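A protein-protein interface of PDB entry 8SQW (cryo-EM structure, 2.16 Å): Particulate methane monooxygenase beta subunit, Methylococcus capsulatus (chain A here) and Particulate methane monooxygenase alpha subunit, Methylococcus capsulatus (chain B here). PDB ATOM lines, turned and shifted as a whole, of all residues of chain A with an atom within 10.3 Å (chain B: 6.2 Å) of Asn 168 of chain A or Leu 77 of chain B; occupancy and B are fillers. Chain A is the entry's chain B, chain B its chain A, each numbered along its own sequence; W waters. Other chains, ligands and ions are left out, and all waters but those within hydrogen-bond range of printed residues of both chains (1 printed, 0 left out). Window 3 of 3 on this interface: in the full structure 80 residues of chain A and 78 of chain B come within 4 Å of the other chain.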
ATOM      1  N   VAL A 165      24.647  11.821 -38.000  1.00  0.00           N
ATOM      2  CA  VAL A 165      25.565  12.326 -36.987  1.00  0.00           C
ATOM      3  C   VAL A 165      26.495  11.197 -36.570  1.00  0.00           C
ATOM      4  O   VAL A 165      26.060  10.059 -36.377  1.00  0.00           O
ATOM      5  CB  VAL A 165      24.820  12.891 -35.762  1.00  0.00           C
ATOM      6  CG1 VAL A 165      25.811  13.343 -34.707  1.00  0.00           C
ATOM      7  CG2 VAL A 165      23.908  14.038 -36.165  1.00  0.00           C
ATOM      8  N   GLU A 166      27.777  11.517 -36.433  1.00  0.00           N
ATOM      9  CA  GLU A 166      28.767  10.578 -35.914  1.00  0.00           C
ATOM     10  C   GLU A 166      28.770  10.716 -34.397  1.00  0.00           C
ATOM     11  O   GLU A 166      29.367  11.644 -33.847  1.00  0.00           O
ATOM     12  CB  GLU A 166      30.138  10.876 -36.511  1.00  0.00           C
ATOM     13  CG  GLU A 166      31.081   9.697 -36.561  1.00  0.00           C
ATOM     14  CD  GLU A 166      31.397   9.144 -35.198  1.00  0.00           C
ATOM     15  OE1 GLU A 166      31.966   9.881 -34.365  1.00  0.00           O
ATOM     16  OE2 GLU A 166      31.058   7.970 -34.960  1.00  0.00           O
ATOM     17  N   TYR A 167      28.098   9.796 -33.711  1.00  0.00           N
ATOM     18  CA  TYR A 167      27.853   9.911 -32.272  1.00  0.00           C
ATOM     19  C   TYR A 167      28.620   8.813 -31.539  1.00  0.00           C
ATOM     20  O   TYR A 167      28.177   7.662 -31.499  1.00  0.00           O
ATOM     21  CB  TYR A 167      26.359   9.835 -31.972  1.00  0.00           C
ATOM     22  CG  TYR A 167      25.986  10.302 -30.583  1.00  0.00           C
ATOM     23  CD1 TYR A 167      25.860  11.654 -30.294  1.00  0.00           C
ATOM     24  CD2 TYR A 167      25.754   9.391 -29.564  1.00  0.00           C
ATOM     25  CE1 TYR A 167      25.516  12.083 -29.029  1.00  0.00           C
ATOM     26  CE2 TYR A 167      25.409   9.812 -28.294  1.00  0.00           C
ATOM     27  CZ  TYR A 167      25.293  11.159 -28.034  1.00  0.00           C
ATOM     28  OH  TYR A 167      24.952  11.582 -26.770  1.00  0.00           O
ATOM     29  N   ASN A 168      29.761   9.188 -30.956  1.00  0.00           N
ATOM     30  CA  ASN A 168      30.554   8.296 -30.103  1.00  0.00           C
ATOM     31  C   ASN A 168      30.894   6.983 -30.809  1.00  0.00           C
ATOM     32  O   ASN A 168      30.776   5.898 -30.240  1.00  0.00           O
ATOM     33  CB  ASN A 168      29.839   8.029 -28.779  1.00  0.00           C
ATOM     34  CG  ASN A 168      29.703   9.278 -27.930  1.00  0.00           C
ATOM     35  OD1 ASN A 168      28.599   9.771 -27.702  1.00  0.00           O
ATOM     36  ND2 ASN A 168      30.828   9.794 -27.456  1.00  0.00           N
ATOM     37  N   GLY A 169      31.324   7.086 -32.065  1.00  0.00           N
ATOM     38  CA  GLY A 169      31.756   5.932 -32.824  1.00  0.00           C
ATOM     39  C   GLY A 169      30.676   5.241 -33.626  1.00  0.00           C
ATOM     40  O   GLY A 169      30.999   4.384 -34.456  1.00  0.00           O
ATOM     41  N   MET A 170      29.409   5.584 -33.416  1.00  0.00           N
ATOM     42  CA  MET A 170      28.297   4.947 -34.103  1.00  0.00           C
ATOM     43  C   MET A 170      27.533   5.978 -34.922  1.00  0.00           C
ATOM     44  O   MET A 170      27.417   7.140 -34.523  1.00  0.00           O
ATOM     45  CB  MET A 170      27.356   4.265 -33.105  1.00  0.00           C
ATOM     46  CG  MET A 170      27.848   2.905 -32.629  1.00  0.00           C
ATOM     47  SD  MET A 170      26.537   1.862 -31.960  1.00  0.00           S
ATOM     48  CE  MET A 170      25.587   1.520 -33.436  1.00  0.00           C
ATOM     49  N   LEU A 171      27.019   5.550 -36.073  1.00  0.00           N
ATOM     50  CA  LEU A 171      26.208   6.425 -36.907  1.00  0.00           C
ATOM     51  C   LEU A 171      24.796   6.494 -36.341  1.00  0.00           C
ATOM     52  O   LEU A 171      24.173   5.458 -36.085  1.00  0.00           O
ATOM     53  CB  LEU A 171      26.182   5.935 -38.352  1.00  0.00           C
ATOM     54  CG  LEU A 171      25.306   6.795 -39.270  1.00  0.00           C
ATOM     55  CD1 LEU A 171      25.962   8.137 -39.519  1.00  0.00           C
ATOM     56  CD2 LEU A 171      25.009   6.097 -40.582  1.00  0.00           C
ATOM     57  N   MET A 172      24.296   7.709 -36.146  1.00  0.00           N
ATOM     58  CA  MET A 172      22.959   7.917 -35.615  1.00  0.00           C
ATOM     59  C   MET A 172      22.340   9.133 -36.284  1.00  0.00           C
ATOM     60  O   MET A 172      23.026  10.115 -36.576  1.00  0.00           O
ATOM     61  CB  MET A 172      22.980   8.112 -34.092  1.00  0.00           C
ATOM     62  CG  MET A 172      23.153   6.833 -33.295  1.00  0.00           C
ATOM     63  SD  MET A 172      23.433   7.141 -31.542  1.00  0.00           S
ATOM     64  CE  MET A 172      21.749   7.238 -30.942  1.00  0.00           C
ATOM     65  N   ASP A 176      17.446   9.647 -33.682  1.00  0.00           N
ATOM     66  CA  ASP A 176      18.036   8.582 -32.879  1.00  0.00           C
ATOM     67  C   ASP A 176      18.716   9.148 -31.641  1.00  0.00           C
ATOM     68  O   ASP A 176      18.566   8.610 -30.537  1.00  0.00           O
ATOM     69  CB  ASP A 176      19.038   7.783 -33.712  1.00  0.00           C
ATOM     70  CG  ASP A 176      18.365   6.849 -34.699  1.00  0.00           C
ATOM     71  OD1 ASP A 176      17.504   6.051 -34.275  1.00  0.00           O
ATOM     72  OD2 ASP A 176      18.700   6.919 -35.899  1.00  0.00           O
ATOM     73  N   ILE A 177      19.465  10.241 -31.803  1.00  0.00           N
ATOM     74  CA  ILE A 177      20.140  10.857 -30.664  1.00  0.00           C
ATOM     75  C   ILE A 177      19.124  11.440 -29.691  1.00  0.00           C
ATOM     76  O   ILE A 177      19.331  11.412 -28.474  1.00  0.00           O
ATOM     77  CB  ILE A 177      21.142  11.918 -31.147  1.00  0.00           C
ATOM     78  CG1 ILE A 177      22.244  11.259 -31.968  1.00  0.00           C
ATOM     79  CG2 ILE A 177      21.761  12.653 -29.972  1.00  0.00           C
ATOM     80  CD1 ILE A 177      23.054  12.230 -32.750  1.00  0.00           C
ATOM     81  N   TYR A 180      17.859   8.576 -27.722  1.00  0.00           N
ATOM     82  CA  TYR A 180      18.908   8.109 -26.822  1.00  0.00           C
ATOM     83  C   TYR A 180      19.072   9.027 -25.619  1.00  0.00           C
ATOM     84  O   TYR A 180      19.117   8.561 -24.475  1.00  0.00           O
ATOM     85  CB  TYR A 180      20.221   7.994 -27.594  1.00  0.00           C
ATOM     86  CG  TYR A 180      21.344   7.342 -26.829  1.00  0.00           C
ATOM     87  CD1 TYR A 180      21.162   6.119 -26.200  1.00  0.00           C
ATOM     88  CD2 TYR A 180      22.590   7.943 -26.751  1.00  0.00           C
ATOM     89  CE1 TYR A 180      22.191   5.520 -25.504  1.00  0.00           C
ATOM     90  CE2 TYR A 180      23.623   7.350 -26.059  1.00  0.00           C
ATOM     91  CZ  TYR A 180      23.418   6.139 -25.439  1.00  0.00           C
ATOM     92  OH  TYR A 180      24.451   5.552 -24.752  1.00  0.00           O
ATOM     93  N   ASN A 181      19.161  10.332 -25.857  1.00  0.00           N
ATOM     94  CA  ASN A 181      19.443  11.312 -24.815  1.00  0.00           C
ATOM     95  C   ASN A 181      18.264  11.481 -23.869  1.00  0.00           C
ATOM     96  O   ASN A 181      18.418  11.365 -22.651  1.00  0.00           O
ATOM     97  CB  ASN A 181      19.801  12.665 -25.437  1.00  0.00           C
ATOM     98  CG  ASN A 181      21.173  12.669 -26.075  1.00  0.00           C
ATOM     99  OD1 ASN A 181      21.546  13.624 -26.752  1.00  0.00           O
ATOM    100  ND2 ASN A 181      21.932  11.604 -25.864  1.00  0.00           N
ATOM    101  N   LYS B  69      24.005  10.809 -22.081  1.00  0.00           N
ATOM    102  CA  LYS B  69      25.029  11.148 -23.063  1.00  0.00           C
ATOM    103  C   LYS B  69      25.635   9.889 -23.670  1.00  0.00           C
ATOM    104  O   LYS B  69      25.772   9.775 -24.892  1.00  0.00           O
ATOM    105  CB  LYS B  69      26.111  12.013 -22.416  1.00  0.00           C
ATOM    106  CG  LYS B  69      25.820  13.504 -22.457  1.00  0.00           C
ATOM    107  CD  LYS B  69      25.414  13.959 -23.848  1.00  0.00           C
ATOM    108  CE  LYS B  69      26.581  13.890 -24.819  1.00  0.00           C
ATOM    109  NZ  LYS B  69      26.290  14.597 -26.096  1.00  0.00           N
ATOM    110  N   GLU B  70      25.990   8.923 -22.825  1.00  0.00           N
ATOM    111  CA  GLU B  70      26.601   7.686 -23.284  1.00  0.00           C
ATOM    112  C   GLU B  70      26.172   6.550 -22.368  1.00  0.00           C
ATOM    113  O   GLU B  70      25.820   6.759 -21.204  1.00  0.00           O
ATOM    114  CB  GLU B  70      28.130   7.778 -23.314  1.00  0.00           C
ATOM    115  CG  GLU B  70      28.700   8.689 -24.383  1.00  0.00           C
ATOM    116  CD  GLU B  70      29.747   9.637 -23.840  1.00  0.00           C
ATOM    117  OE1 GLU B  70      30.647   9.173 -23.108  1.00  0.00           O
ATOM    118  OE2 GLU B  70      29.672  10.846 -24.141  1.00  0.00           O
ATOM    119  N   SER B  71      26.213   5.338 -22.910  1.00  0.00           N
ATOM    120  CA  SER B  71      25.978   4.127 -22.136  1.00  0.00           C
ATOM    121  C   SER B  71      26.817   3.015 -22.745  1.00  0.00           C
ATOM    122  O   SER B  71      26.877   2.888 -23.971  1.00  0.00           O
ATOM    123  CB  SER B  71      24.496   3.740 -22.123  1.00  0.00           C
ATOM    124  OG  SER B  71      23.966   3.705 -23.435  1.00  0.00           O
ATOM    125  N   TYR B  72      27.462   2.223 -21.896  1.00  0.00           N
ATOM    126  CA  TYR B  72      28.366   1.179 -22.348  1.00  0.00           C
ATOM    127  C   TYR B  72      28.052  -0.132 -21.646  1.00  0.00           C
ATOM    128  O   TYR B  72      27.730  -0.148 -20.456  1.00  0.00           O
ATOM    129  CB  TYR B  72      29.833   1.552 -22.092  1.00  0.00           C
ATOM    130  CG  TYR B  72      30.267   2.849 -22.729  1.00  0.00           C
ATOM    131  CD1 TYR B  72      30.060   4.061 -22.088  1.00  0.00           C
ATOM    132  CD2 TYR B  72      30.881   2.863 -23.971  1.00  0.00           C
ATOM    133  CE1 TYR B  72      30.454   5.247 -22.663  1.00  0.00           C
ATOM    134  CE2 TYR B  72      31.279   4.049 -24.558  1.00  0.00           C
ATOM    135  CZ  TYR B  72      31.061   5.236 -23.899  1.00  0.00           C
ATOM    136  OH  TYR B  72      31.454   6.419 -24.476  1.00  0.00           O
ATOM    137  N   ILE B  73      28.137  -1.226 -22.395  1.00  0.00           N
ATOM    138  CA  ILE B  73      28.163  -2.571 -21.837  1.00  0.00           C
ATOM    139  C   ILE B  73      29.471  -3.204 -22.286  1.00  0.00           C
ATOM    140  O   ILE B  73      29.724  -3.332 -23.492  1.00  0.00           O
ATOM    141  CB  ILE B  73      26.954  -3.406 -22.283  1.00  0.00           C
ATOM    142  CG1 ILE B  73      25.658  -2.787 -21.755  1.00  0.00           C
ATOM    143  CG2 ILE B  73      27.108  -4.849 -21.820  1.00  0.00           C
ATOM    144  CD1 ILE B  73      24.482  -3.737 -21.744  1.00  0.00           C
ATOM    145  N   GLY B  75      32.840  -2.334 -22.960  1.00  0.00           N
ATOM    146  CA  GLY B  75      33.564  -1.097 -23.164  1.00  0.00           C
ATOM    147  C   GLY B  75      33.072  -0.342 -24.382  1.00  0.00           C
ATOM    148  O   GLY B  75      33.677   0.648 -24.798  1.00  0.00           O
ATOM    149  N   GLN B  76      31.966  -0.804 -24.957  1.00  0.00           N
ATOM    150  CA  GLN B  76      31.457  -0.296 -26.221  1.00  0.00           C
ATOM    151  C   GLN B  76      30.082   0.335 -26.041  1.00  0.00           C
ATOM    152  O   GLN B  76      29.279  -0.120 -25.222  1.00  0.00           O
ATOM    153  CB  GLN B  76      31.408  -1.416 -27.260  1.00  0.00           C
ATOM    154  CG  GLN B  76      30.470  -2.546 -26.906  1.00  0.00           C
ATOM    155  CD  GLN B  76      29.719  -3.068 -28.106  1.00  0.00           C
ATOM    156  OE1 GLN B  76      28.751  -2.458 -28.553  1.00  0.00           O
ATOM    157  NE2 GLN B  76      30.161  -4.202 -28.636  1.00  0.00           N
ATOM    158  N   LEU B  77      29.825   1.391 -26.813  1.00  0.00           N
ATOM    159  CA  LEU B  77      28.587   2.146 -26.681  1.00  0.00           C
ATOM    160  C   LEU B  77      27.389   1.311 -27.113  1.00  0.00           C
ATOM    161  O   LEU B  77      27.453   0.559 -28.088  1.00  0.00           O
ATOM    162  CB  LEU B  77      28.670   3.426 -27.513  1.00  0.00           C
ATOM    163  CG  LEU B  77      27.571   4.467 -27.303  1.00  0.00           C
ATOM    164  CD1 LEU B  77      28.030   5.531 -26.322  1.00  0.00           C
ATOM    165  CD2 LEU B  77      27.173   5.091 -28.627  1.00  0.00           C
ATOM    166  N   VAL B  78      26.287   1.451 -26.382  1.00  0.00           N
ATOM    167  CA  VAL B  78      25.099   0.638 -26.630  1.00  0.00           C
ATOM    168  C   VAL B  78      23.865   1.526 -26.755  1.00  0.00           C
ATOM    169  O   VAL B  78      22.986   1.498 -25.883  1.00  0.00           O
ATOM    170  CB  VAL B  78      24.921  -0.421 -25.529  1.00  0.00           C
ATOM    171  CG1 VAL B  78      25.922  -1.540 -25.725  1.00  0.00           C
ATOM    172  CG2 VAL B  78      25.109   0.195 -24.151  1.00  0.00           C
ATOM    173  N   PRO B  79      23.739   2.316 -27.828  1.00  0.00           N
ATOM    174  CA  PRO B  79      22.526   3.128 -27.995  1.00  0.00           C
ATOM    175  C   PRO B  79      21.308   2.321 -28.406  1.00  0.00           C
ATOM    176  O   PRO B  79      20.197   2.866 -28.392  1.00  0.00           O
ATOM    177  CB  PRO B  79      22.922   4.124 -29.089  1.00  0.00           C
ATOM    178  CG  PRO B  79      23.909   3.376 -29.909  1.00  0.00           C
ATOM    179  CD  PRO B  79      24.662   2.469 -28.966  1.00  0.00           C
ATOM    180  N   ARG B  80      21.478   1.059 -28.774  1.00  0.00           N
ATOM    181  CA  ARG B  80      20.394   0.189 -29.190  1.00  0.00           C
ATOM    182  C   ARG B  80      20.253  -0.963 -28.199  1.00  0.00           C
ATOM    183  O   ARG B  80      21.012  -1.084 -27.235  1.00  0.00           O
ATOM    184  CB  ARG B  80      20.637  -0.331 -30.607  1.00  0.00           C
ATOM    185  CG  ARG B  80      21.202   0.710 -31.560  1.00  0.00           C
ATOM    186  CD  ARG B  80      20.825   0.401 -32.991  1.00  0.00           C
ATOM    187  NE  ARG B  80      21.890   0.728 -33.932  1.00  0.00           N
ATOM    188  CZ  ARG B  80      22.451  -0.145 -34.757  1.00  0.00           C
ATOM    189  NH1 ARG B  80      22.090  -1.415 -34.767  1.00  0.00           N
ATOM    190  NH2 ARG B  80      23.395   0.269 -35.594  1.00  0.00           N
ATOM    191  N   MET B 237      22.013  -5.324 -30.941  1.00  0.00           N
ATOM    192  CA  MET B 237      23.449  -5.455 -31.133  1.00  0.00           C
ATOM    193  C   MET B 237      23.937  -6.701 -30.404  1.00  0.00           C
ATOM    194  O   MET B 237      23.746  -6.831 -29.190  1.00  0.00           O
ATOM    195  CB  MET B 237      24.170  -4.210 -30.626  1.00  0.00           C
ATOM    196  CG  MET B 237      24.017  -3.008 -31.545  1.00  0.00           C
ATOM    197  SD  MET B 237      24.591  -1.475 -30.796  1.00  0.00           S
ATOM    198  CE  MET B 237      26.241  -1.952 -30.309  1.00  0.00           C
ATOM    199  N   MET B 240      28.071  -8.705 -27.139  1.00  0.00           N
ATOM    200  CA  MET B 240      28.445  -7.983 -25.928  1.00  0.00           C
ATOM    201  C   MET B 240      29.547  -8.769 -25.232  1.00  0.00           C
ATOM    202  O   MET B 240      29.427  -9.981 -25.040  1.00  0.00           O
ATOM    203  CB  MET B 240      27.241  -7.791 -25.013  1.00  0.00           C
ATOM    204  CG  MET B 240      26.094  -6.987 -25.613  1.00  0.00           C
ATOM    205  SD  MET B 240      26.505  -5.260 -25.941  1.00  0.00           S
ATOM    206  CE  MET B 240      26.958  -5.317 -27.675  1.00  0.00           C
HETATM  207  O   HOH W   1      24.115   2.733 -36.852  1.00  0.00           O
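The backbone carbonyl oxygen (O) of Lys 69 of chain B lies within hydrogen-bond range of the side-chain hydroxyl (OH) of Tyr 167 of chain A (2.7 Å). OH of Tyr 180 of chain A is in hydrogen-bond range of N of Ser 71 of chain B (2.6 Å).
The backbone NH of Val 78 of chain B sits at hydrogen-bond distance from the backbone carbonyl oxygen of Ser 71 of chain B (2.9 Å). N of Val 165 of chain A lies within hydrogen-bond range of O of Met 172 of chain A. The side-chain hydroxyl of Tyr 72 of chain B is in hydrogen-bond range of the side-chain carboxylate of Glu 70 of chain B, at 3.2 Å. OE2 of Glu 166 of chain A sits at hydrogen-bond distance from N of Met 170 of chain A (3.3 Å). The side-chain hydroxyl (OH) of Tyr 167 of chain A is in hydrogen-bond range of the side-chain amide nitrogen (ND2) of Asn 181 of chain A.
CD2 of Leu 77 of chain B touches O of Tyr 167 of chain A (3.98 Å). Lys 69 of chain B touches Asn 168 of chain A (O to OD1, 3.99 Å). OD1 of Asn 168 of chain A touches CG of Glu 70 of chain B (3.5 Å). Asn 168 of chain A touches Leu 77 of chain B (CB to CD1, 3.9 Å). SD of Met 170 of chain A touches CD of Pro 79 of chain B, 3.6 Å away. CE of Met 170 of chain A touches NH2 of Arg 80 of chain B, at 3.3 Å. Met 172 of chain A touches Pro 79 of chain B. Tyr 180 of chain A touches Glu 70 of chain B (OH to C, 3.1 Å). OH of Tyr 180 of chain A touches CD1 of Leu 77 of chain B, 3.9 Å away. Pro 79 of chain B touches Tyr 180 of chain A.
Of the printed residues of chain B, Tyr 167 of chain A touches Lys 69 (2.7 Å) and Leu 77 (3.98 Å). Printed residues of chain B within 4 Å of Asn 168 of chain A: Lys 69 (3.99 Å), Glu 70 (3.5 Å) and Leu 77 (3.9 Å). Of the printed residues of chain B, Met 170 of chain A touches Pro 79 (3.6 Å) and Arg 80 (3.3 Å). Ile 177 of chain A touches none of the printed residues of chain B. Glu 70 of chain B touches two residues of chain A. Ser 71 of chain B touches one residue of chain A. No residue of chain A comes within 4 Å of Gly 75 of chain B. Of the printed residues of chain A, Leu 77 of chain B touches Tyr 167 (3.98 Å), Asn 168 (3.9 Å) and Tyr 180 (3.9 Å). No residue of chain A comes within 4 Å of Val 78 of chain B. Of the printed residues of chain A, Arg 80 of chain B touches Met 170 (3.3 Å). Met 237 of chain B touches none of the printed residues of chain A. The nearest printed residue of chain B that does not touch Asn 168 of chain A is Tyr 72 of chain B (4.5 Å). The nearest printed residue of chain A that does not touch Leu 77 of chain B is Met 170 of chain A (4.2 Å). The nearest printed residue of chain A that does not touch Arg 80 of chain B is Leu 171 of chain A (5.3 Å).
Of the 12 printed residues of chain A, 5 touch a printed residue of chain B. Printed residues of chain A that touch a printed residue of chain B: Tyr 167, Asn 168, Met 170, Met 172 and Tyr 180. Hydrophobic or aromatic side chains of chain A within 4 Å of the printed part of chain B: Tyr 167, Met 170, Met 172 and Tyr 180. Of the 13 printed residues of chain B, 6 touch a printed residue of chain A. Printed residues of chain B that touch a printed residue of chain A: Lys 69, Glu 70, Ser 71, Leu 77, Pro 79 and Arg 80. Hydrophobic or aromatic side chains of chain B that line the printed part of chain A: Leu 77 and Pro 79.
Water W1 bridges the backbone carbonyl oxygen of Leu 171 of chain A (2.8 Å) and the guanidinium group of Arg 80 of chain B (2.9 Å).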
